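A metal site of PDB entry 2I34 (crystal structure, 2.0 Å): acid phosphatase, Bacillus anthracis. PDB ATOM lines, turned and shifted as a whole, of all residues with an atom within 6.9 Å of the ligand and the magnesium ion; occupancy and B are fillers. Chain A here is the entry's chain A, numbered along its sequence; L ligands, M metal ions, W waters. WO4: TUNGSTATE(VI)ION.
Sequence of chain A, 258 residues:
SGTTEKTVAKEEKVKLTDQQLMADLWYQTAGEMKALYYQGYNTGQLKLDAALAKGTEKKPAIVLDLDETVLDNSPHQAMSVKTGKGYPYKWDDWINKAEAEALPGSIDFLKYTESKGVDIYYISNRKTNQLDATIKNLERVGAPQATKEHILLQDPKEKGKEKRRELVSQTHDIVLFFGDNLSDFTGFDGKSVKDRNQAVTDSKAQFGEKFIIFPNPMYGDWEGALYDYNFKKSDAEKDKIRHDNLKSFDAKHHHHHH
OD1 of Asp 65 is bound to W of the ligand (2.5 Å). An oxygen (O3) of the ligand sits close to the side-chain hydroxyl (OG) of Ser 124 (2.4 Å). The side-chain amino group (NZ) of Lys 161 sits close to an oxygen (O4) of the ligand.
OD1 of Asp 65 lies close to NZ of Lys 161 (2.8 Å). OG1 of Thr 69 sits close to OD2 of Asp 65 (2.9 Å). N of Asp 180 lies within hydrogen-bond range of OD2 of Asp 184 (3.1 Å). N of Arg 126 sits at hydrogen-bond distance from OG of Ser 124 (3.2 Å). NH1 of Arg 164 lies within hydrogen-bond range of O of Ser 124 (2.8 Å). The side-chain amino group of Lys 161 lies within salt-bridge range of the side-chain carboxylate of Asp 184 (3.0 Å). O of Ile 123 sits at hydrogen-bond distance from NZ of Lys 161 (2.9 Å). The guanidinium group (NH2) of Arg 126 lies within hydrogen-bond range of the side-chain amide oxygen (OD1) of Asn 73, 3.5 Å away.
O3 of the ligand lies close to N of Leu 66, at 3.1 Å. The backbone NH (N) of Asn 125 lies close to an oxygen (O4) of the ligand. Residues that only touch the ligand: Arg 126 (3.8 Å). Hydrophobic or aromatic side chains within 4 Å of the ligand: Leu 66.
Merely in contact with the magnesium ion: Asp 184. Along chain A the residues within 4 Å of the magnesium ion span positions 65 to 184.
The magnesium ion is bound by O2 of the ligand (1.8 Å), OD2 of Asp 65 (2.0 Å), OD1 of Asp 180 (2.1 Å), water W2 (2.1 Å), O of Asp 67 (2.1 Å) and water W3 (2.1 Å).
Water W3 bridges OD2 of Asp 180 and OH of Tyr 219.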
ATOM      1  N   LEU A  64     -19.317  30.003  18.814  1.00  0.00           N
ATOM      2  CA  LEU A  64     -19.593  28.907  17.915  1.00  0.00           C
ATOM      3  C   LEU A  64     -19.739  27.606  18.678  1.00  0.00           C
ATOM      4  O   LEU A  64     -18.962  27.308  19.602  1.00  0.00           O
ATOM      5  CB  LEU A  64     -18.478  28.726  16.880  1.00  0.00           C
ATOM      6  CG  LEU A  64     -17.984  29.977  16.143  1.00  0.00           C
ATOM      7  CD1 LEU A  64     -16.755  30.558  16.829  1.00  0.00           C
ATOM      8  CD2 LEU A  64     -17.719  29.639  14.673  1.00  0.00           C
ATOM      9  N   ASP A  65     -20.734  26.826  18.262  1.00  0.00           N
ATOM     10  CA  ASP A  65     -20.777  25.393  18.511  1.00  0.00           C
ATOM     11  C   ASP A  65     -19.599  24.714  17.803  1.00  0.00           C
ATOM     12  O   ASP A  65     -19.032  25.280  16.860  1.00  0.00           O
ATOM     13  CB  ASP A  65     -22.087  24.843  17.938  1.00  0.00           C
ATOM     14  CG  ASP A  65     -22.171  23.365  18.043  1.00  0.00           C
ATOM     15  OD1 ASP A  65     -22.122  22.872  19.185  1.00  0.00           O
ATOM     16  OD2 ASP A  65     -22.282  22.683  16.982  1.00  0.00           O
ATOM     17  N   LEU A  66     -19.233  23.502  18.244  1.00  0.00           N
ATOM     18  CA  LEU A  66     -18.184  22.715  17.542  1.00  0.00           C
ATOM     19  C   LEU A  66     -18.686  21.657  16.551  1.00  0.00           C
ATOM     20  O   LEU A  66     -18.414  21.756  15.361  1.00  0.00           O
ATOM     21  CB  LEU A  66     -17.208  22.074  18.540  1.00  0.00           C
ATOM     22  CG  LEU A  66     -16.214  23.055  19.165  1.00  0.00           C
ATOM     23  CD1 LEU A  66     -15.327  22.355  20.209  1.00  0.00           C
ATOM     24  CD2 LEU A  66     -15.345  23.711  18.097  1.00  0.00           C
ATOM     25  N   ASP A  67     -19.366  20.634  17.053  1.00  0.00           N
ATOM     26  CA  ASP A  67     -19.745  19.482  16.227  1.00  0.00           C
ATOM     27  C   ASP A  67     -20.799  19.859  15.193  1.00  0.00           C
ATOM     28  O   ASP A  67     -21.871  20.361  15.541  1.00  0.00           O
ATOM     29  CB  ASP A  67     -20.223  18.308  17.098  1.00  0.00           C
ATOM     30  CG  ASP A  67     -19.160  17.869  18.095  1.00  0.00           C
ATOM     31  OD1 ASP A  67     -17.963  17.836  17.722  1.00  0.00           O
ATOM     32  OD2 ASP A  67     -19.490  17.631  19.269  1.00  0.00           O
ATOM     33  N   GLU A  68     -20.461  19.629  13.924  1.00  0.00           N
ATOM     34  CA  GLU A  68     -21.302  19.974  12.782  1.00  0.00           C
ATOM     35  C   GLU A  68     -21.447  21.499  12.582  1.00  0.00           C
ATOM     36  O   GLU A  68     -22.294  21.942  11.803  1.00  0.00           O
ATOM     37  CB  GLU A  68     -22.647  19.249  12.848  1.00  0.00           C
ATOM     38  CG  GLU A  68     -22.572  17.788  12.326  1.00  0.00           C
ATOM     39  CD  GLU A  68     -21.400  17.003  12.913  1.00  0.00           C
ATOM     40  OE1 GLU A  68     -21.434  16.611  14.102  1.00  0.00           O
ATOM     41  OE2 GLU A  68     -20.434  16.791  12.156  1.00  0.00           O
ATOM     42  N   THR A  69     -20.583  22.267  13.234  1.00  0.00           N
ATOM     43  CA  THR A  69     -20.447  23.691  12.974  1.00  0.00           C
ATOM     44  C   THR A  69     -19.011  23.987  12.511  1.00  0.00           C
ATOM     45  O   THR A  69     -18.818  24.515  11.419  1.00  0.00           O
ATOM     46  CB  THR A  69     -20.811  24.514  14.206  1.00  0.00           C
ATOM     47  OG1 THR A  69     -22.172  24.255  14.531  1.00  0.00           O
ATOM     48  CG2 THR A  69     -20.652  25.982  13.952  1.00  0.00           C
ATOM     49  N   ASN A  73     -18.047  15.532  12.283  1.00  0.00           N
ATOM     50  CA  ASN A  73     -18.109  14.239  12.947  1.00  0.00           C
ATOM     51  C   ASN A  73     -18.848  13.199  12.134  1.00  0.00           C
ATOM     52  O   ASN A  73     -19.163  12.124  12.633  1.00  0.00           O
ATOM     53  CB  ASN A  73     -18.794  14.386  14.310  1.00  0.00           C
ATOM     54  CG  ASN A  73     -18.088  15.355  15.202  1.00  0.00           C
ATOM     55  OD1 ASN A  73     -17.036  15.066  15.784  1.00  0.00           O
ATOM     56  ND2 ASN A  73     -18.652  16.528  15.322  1.00  0.00           N
ATOM     57  N   TYR A  87     -25.278   6.233  17.825  1.00  0.00           N
ATOM     58  CA  TYR A  87     -24.669   7.129  18.796  1.00  0.00           C
ATOM     59  C   TYR A  87     -25.316   6.889  20.158  1.00  0.00           C
ATOM     60  O   TYR A  87     -26.520   6.638  20.233  1.00  0.00           O
ATOM     61  CB  TYR A  87     -24.854   8.585  18.322  1.00  0.00           C
ATOM     62  CG  TYR A  87     -24.544   9.614  19.376  1.00  0.00           C
ATOM     63  CD1 TYR A  87     -25.495   9.965  20.336  1.00  0.00           C
ATOM     64  CD2 TYR A  87     -23.294  10.231  19.426  1.00  0.00           C
ATOM     65  CE1 TYR A  87     -25.207  10.889  21.323  1.00  0.00           C
ATOM     66  CE2 TYR A  87     -23.007  11.154  20.412  1.00  0.00           C
ATOM     67  CZ  TYR A  87     -23.962  11.467  21.359  1.00  0.00           C
ATOM     68  OH  TYR A  87     -23.685  12.393  22.332  1.00  0.00           O
ATOM     69  N   TRP A  91     -18.485   6.829  20.510  1.00  0.00           N
ATOM     70  CA  TRP A  91     -18.402   8.267  20.382  1.00  0.00           C
ATOM     71  C   TRP A  91     -17.146   8.778  21.097  1.00  0.00           C
ATOM     72  O   TRP A  91     -16.383   9.576  20.541  1.00  0.00           O
ATOM     73  CB  TRP A  91     -19.671   8.948  20.906  1.00  0.00           C
ATOM     74  CG  TRP A  91     -19.580  10.435  20.906  1.00  0.00           C
ATOM     75  CD1 TRP A  91     -19.473  11.245  21.993  1.00  0.00           C
ATOM     76  CD2 TRP A  91     -19.586  11.302  19.762  1.00  0.00           C
ATOM     77  NE1 TRP A  91     -19.404  12.551  21.608  1.00  0.00           N
ATOM     78  CE2 TRP A  91     -19.472  12.618  20.244  1.00  0.00           C
ATOM     79  CE3 TRP A  91     -19.669  11.082  18.388  1.00  0.00           C
ATOM     80  CZ2 TRP A  91     -19.436  13.717  19.395  1.00  0.00           C
ATOM     81  CZ3 TRP A  91     -19.648  12.163  17.540  1.00  0.00           C
ATOM     82  CH2 TRP A  91     -19.526  13.480  18.055  1.00  0.00           C
ATOM     83  N   ILE A 123     -18.418  27.086  22.374  1.00  0.00           N
ATOM     84  CA  ILE A 123     -19.319  26.614  23.390  1.00  0.00           C
ATOM     85  C   ILE A 123     -19.944  25.332  22.822  1.00  0.00           C
ATOM     86  O   ILE A 123     -20.757  25.407  21.913  1.00  0.00           O
ATOM     87  CB  ILE A 123     -20.370  27.682  23.777  1.00  0.00           C
ATOM     88  CG1 ILE A 123     -19.654  28.909  24.332  1.00  0.00           C
ATOM     89  CG2 ILE A 123     -21.352  27.137  24.812  1.00  0.00           C
ATOM     90  CD1 ILE A 123     -20.594  30.000  24.923  1.00  0.00           C
ATOM     91  N   SER A 124     -19.566  24.202  23.425  1.00  0.00           N
ATOM     92  CA  SER A 124     -19.835  22.875  22.894  1.00  0.00           C
ATOM     93  C   SER A 124     -20.320  21.932  24.009  1.00  0.00           C
ATOM     94  O   SER A 124     -19.833  21.995  25.139  1.00  0.00           O
ATOM     95  CB  SER A 124     -18.548  22.300  22.280  1.00  0.00           C
ATOM     96  OG  SER A 124     -18.697  20.929  21.937  1.00  0.00           O
ATOM     97  N   ASN A 125     -21.258  21.059  23.654  1.00  0.00           N
ATOM     98  CA  ASN A 125     -21.766  20.047  24.550  1.00  0.00           C
ATOM     99  C   ASN A 125     -20.963  18.744  24.575  1.00  0.00           C
ATOM    100  O   ASN A 125     -21.384  17.780  25.188  1.00  0.00           O
ATOM    101  CB  ASN A 125     -23.244  19.803  24.290  1.00  0.00           C
ATOM    102  CG  ASN A 125     -24.099  20.936  24.827  1.00  0.00           C
ATOM    103  OD1 ASN A 125     -23.604  21.804  25.543  1.00  0.00           O
ATOM    104  ND2 ASN A 125     -25.385  20.920  24.498  1.00  0.00           N
ATOM    105  N   ARG A 126     -19.794  18.740  23.942  1.00  0.00           N
ATOM    106  CA  ARG A 126     -18.721  17.841  24.386  1.00  0.00           C
ATOM    107  C   ARG A 126     -18.554  18.017  25.878  1.00  0.00           C
ATOM    108  O   ARG A 126     -18.785  19.110  26.388  1.00  0.00           O
ATOM    109  CB  ARG A 126     -17.397  18.149  23.681  1.00  0.00           C
ATOM    110  CG  ARG A 126     -17.439  17.808  22.215  1.00  0.00           C
ATOM    111  CD  ARG A 126     -16.145  18.190  21.500  1.00  0.00           C
ATOM    112  NE  ARG A 126     -16.163  17.725  20.114  1.00  0.00           N
ATOM    113  CZ  ARG A 126     -15.125  17.196  19.475  1.00  0.00           C
ATOM    114  NH1 ARG A 126     -13.962  17.049  20.082  1.00  0.00           N
ATOM    115  NH2 ARG A 126     -15.262  16.772  18.213  1.00  0.00           N
ATOM    116  N   LEU A 153     -16.883  23.714  27.597  1.00  0.00           N
ATOM    117  CA  LEU A 153     -17.577  22.438  27.440  1.00  0.00           C
ATOM    118  C   LEU A 153     -18.606  22.236  28.534  1.00  0.00           C
ATOM    119  O   LEU A 153     -18.670  23.018  29.490  1.00  0.00           O
ATOM    120  CB  LEU A 153     -16.568  21.281  27.404  1.00  0.00           C
ATOM    121  CG  LEU A 153     -15.482  21.400  26.326  1.00  0.00           C
ATOM    122  CD1 LEU A 153     -14.636  20.127  26.229  1.00  0.00           C
ATOM    123  CD2 LEU A 153     -16.072  21.759  24.939  1.00  0.00           C
ATOM    124  N   LYS A 161     -26.711  25.348  27.022  1.00  0.00           N
ATOM    125  CA  LYS A 161     -25.518  26.220  26.950  1.00  0.00           C
ATOM    126  C   LYS A 161     -25.699  27.638  27.511  1.00  0.00           C
ATOM    127  O   LYS A 161     -24.733  28.432  27.534  1.00  0.00           O
ATOM    128  CB  LYS A 161     -25.048  26.331  25.506  1.00  0.00           C
ATOM    129  CG  LYS A 161     -24.593  25.026  24.903  1.00  0.00           C
ATOM    130  CD  LYS A 161     -24.369  25.187  23.402  1.00  0.00           C
ATOM    131  CE  LYS A 161     -23.705  23.945  22.838  1.00  0.00           C
ATOM    132  NZ  LYS A 161     -23.317  24.086  21.424  1.00  0.00           N
ATOM    133  N   ARG A 164     -23.072  29.132  29.919  1.00  0.00           N
ATOM    134  CA  ARG A 164     -21.832  29.543  29.271  1.00  0.00           C
ATOM    135  C   ARG A 164     -21.997  30.802  28.415  1.00  0.00           C
ATOM    136  O   ARG A 164     -21.120  31.657  28.388  1.00  0.00           O
ATOM    137  CB  ARG A 164     -21.231  28.383  28.451  1.00  0.00           C
ATOM    138  CG  ARG A 164     -20.610  27.325  29.358  1.00  0.00           C
ATOM    139  CD  ARG A 164     -20.407  26.020  28.644  1.00  0.00           C
ATOM    140  NE  ARG A 164     -21.636  25.232  28.589  1.00  0.00           N
ATOM    141  CZ  ARG A 164     -21.867  24.252  27.718  1.00  0.00           C
ATOM    142  NH1 ARG A 164     -20.994  23.922  26.790  1.00  0.00           N
ATOM    143  NH2 ARG A 164     -23.014  23.604  27.767  1.00  0.00           N
ATOM    144  N   GLY A 179     -24.095  27.898  14.717  1.00  0.00           N
ATOM    145  CA  GLY A 179     -24.497  26.546  15.109  1.00  0.00           C
ATOM    146  C   GLY A 179     -25.327  25.792  14.088  1.00  0.00           C
ATOM    147  O   GLY A 179     -25.814  26.368  13.094  1.00  0.00           O
ATOM    148  N   ASP A 180     -25.471  24.491  14.322  1.00  0.00           N
ATOM    149  CA  ASP A 180     -26.314  23.623  13.476  1.00  0.00           C
ATOM    150  C   ASP A 180     -27.589  23.197  14.203  1.00  0.00           C
ATOM    151  O   ASP A 180     -28.425  22.495  13.628  1.00  0.00           O
ATOM    152  CB  ASP A 180     -25.534  22.351  13.076  1.00  0.00           C
ATOM    153  CG  ASP A 180     -25.175  21.489  14.277  1.00  0.00           C
ATOM    154  OD1 ASP A 180     -24.307  21.941  15.073  1.00  0.00           O
ATOM    155  OD2 ASP A 180     -25.759  20.382  14.451  1.00  0.00           O
ATOM    156  N   ASN A 181     -27.715  23.622  15.455  1.00  0.00           N
ATOM    157  CA  ASN A 181     -28.769  23.177  16.353  1.00  0.00           C
ATOM    158  C   ASN A 181     -29.344  24.456  16.958  1.00  0.00           C
ATOM    159  O   ASN A 181     -28.581  25.316  17.364  1.00  0.00           O
ATOM    160  CB  ASN A 181     -28.161  22.234  17.411  1.00  0.00           C
ATOM    161  CG  ASN A 181     -29.182  21.603  18.351  1.00  0.00           C
ATOM    162  OD1 ASN A 181     -30.212  22.186  18.691  1.00  0.00           O
ATOM    163  ND2 ASN A 181     -28.865  20.392  18.834  1.00  0.00           N
ATOM    164  N   SER A 183     -30.577  25.080  19.708  1.00  0.00           N
ATOM    165  CA  SER A 183     -30.116  25.290  21.085  1.00  0.00           C
ATOM    166  C   SER A 183     -28.690  25.844  21.171  1.00  0.00           C
ATOM    167  O   SER A 183     -28.209  26.106  22.261  1.00  0.00           O
ATOM    168  CB  SER A 183     -30.297  24.021  21.938  1.00  0.00           C
ATOM    169  OG  SER A 183     -29.545  22.935  21.444  1.00  0.00           O
ATOM    170  N   ASP A 184     -28.016  26.019  20.023  1.00  0.00           N
ATOM    171  CA  ASP A 184     -26.795  26.809  19.931  1.00  0.00           C
ATOM    172  C   ASP A 184     -27.055  28.332  19.980  1.00  0.00           C
ATOM    173  O   ASP A 184     -26.118  29.145  19.993  1.00  0.00           O
ATOM    174  CB  ASP A 184     -26.001  26.442  18.663  1.00  0.00           C
ATOM    175  CG  ASP A 184     -25.672  24.952  18.549  1.00  0.00           C
ATOM    176  OD1 ASP A 184     -25.630  24.275  19.601  1.00  0.00           O
ATOM    177  OD2 ASP A 184     -25.464  24.437  17.414  1.00  0.00           O
ATOM    178  N   ASN A 216     -27.737  20.309   9.291  1.00  0.00           N
ATOM    179  CA  ASN A 216     -27.411  18.987   9.838  1.00  0.00           C
ATOM    180  C   ASN A 216     -28.648  18.097   9.874  1.00  0.00           C
ATOM    181  O   ASN A 216     -29.357  18.060  10.884  1.00  0.00           O
ATOM    182  CB  ASN A 216     -26.769  19.106  11.225  1.00  0.00           C
ATOM    183  CG  ASN A 216     -26.461  17.755  11.858  1.00  0.00           C
ATOM    184  OD1 ASN A 216     -26.583  16.718  11.226  1.00  0.00           O
ATOM    185  ND2 ASN A 216     -26.057  17.774  13.115  1.00  0.00           N
ATOM    186  N   TYR A 219     -28.633  14.401  12.812  1.00  0.00           N
ATOM    187  CA  TYR A 219     -28.957  14.294  14.211  1.00  0.00           C
ATOM    188  C   TYR A 219     -29.208  15.684  14.816  1.00  0.00           C
ATOM    189  O   TYR A 219     -28.929  16.705  14.175  1.00  0.00           O
ATOM    190  CB  TYR A 219     -27.830  13.569  14.965  1.00  0.00           C
ATOM    191  CG  TYR A 219     -26.573  14.413  15.138  1.00  0.00           C
ATOM    192  CD1 TYR A 219     -25.551  14.395  14.189  1.00  0.00           C
ATOM    193  CD2 TYR A 219     -26.452  15.263  16.231  1.00  0.00           C
ATOM    194  CE1 TYR A 219     -24.427  15.193  14.356  1.00  0.00           C
ATOM    195  CE2 TYR A 219     -25.341  16.066  16.395  1.00  0.00           C
ATOM    196  CZ  TYR A 219     -24.328  16.039  15.466  1.00  0.00           C
ATOM    197  OH  TYR A 219     -23.236  16.871  15.683  1.00  0.00           O
HETATM  198  W   WO4 L   1     -21.883  20.542  19.973  1.00  0.00           W
HETATM  199  O1  WO4 L   1     -21.735  18.655  20.720  1.00  0.00           O
HETATM  200  O2  WO4 L   1     -22.828  20.335  18.191  1.00  0.00           O
HETATM  201  O3  WO4 L   1     -19.936  20.970  19.832  1.00  0.00           O
HETATM  202  O4  WO4 L   1     -22.890  21.520  21.434  1.00  0.00           O
HETATM  203 MG    MG M   1     -23.480  21.051  16.733  1.00  0.00          MG
HETATM  204  O   HOH W   1     -25.420  20.858  20.615  1.00  0.00           O
HETATM  205  O   HOH W   2     -24.988  21.914  17.912  1.00  0.00           O
HETATM  206  O   HOH W   3     -24.584  19.247  16.527  1.00  0.00           O
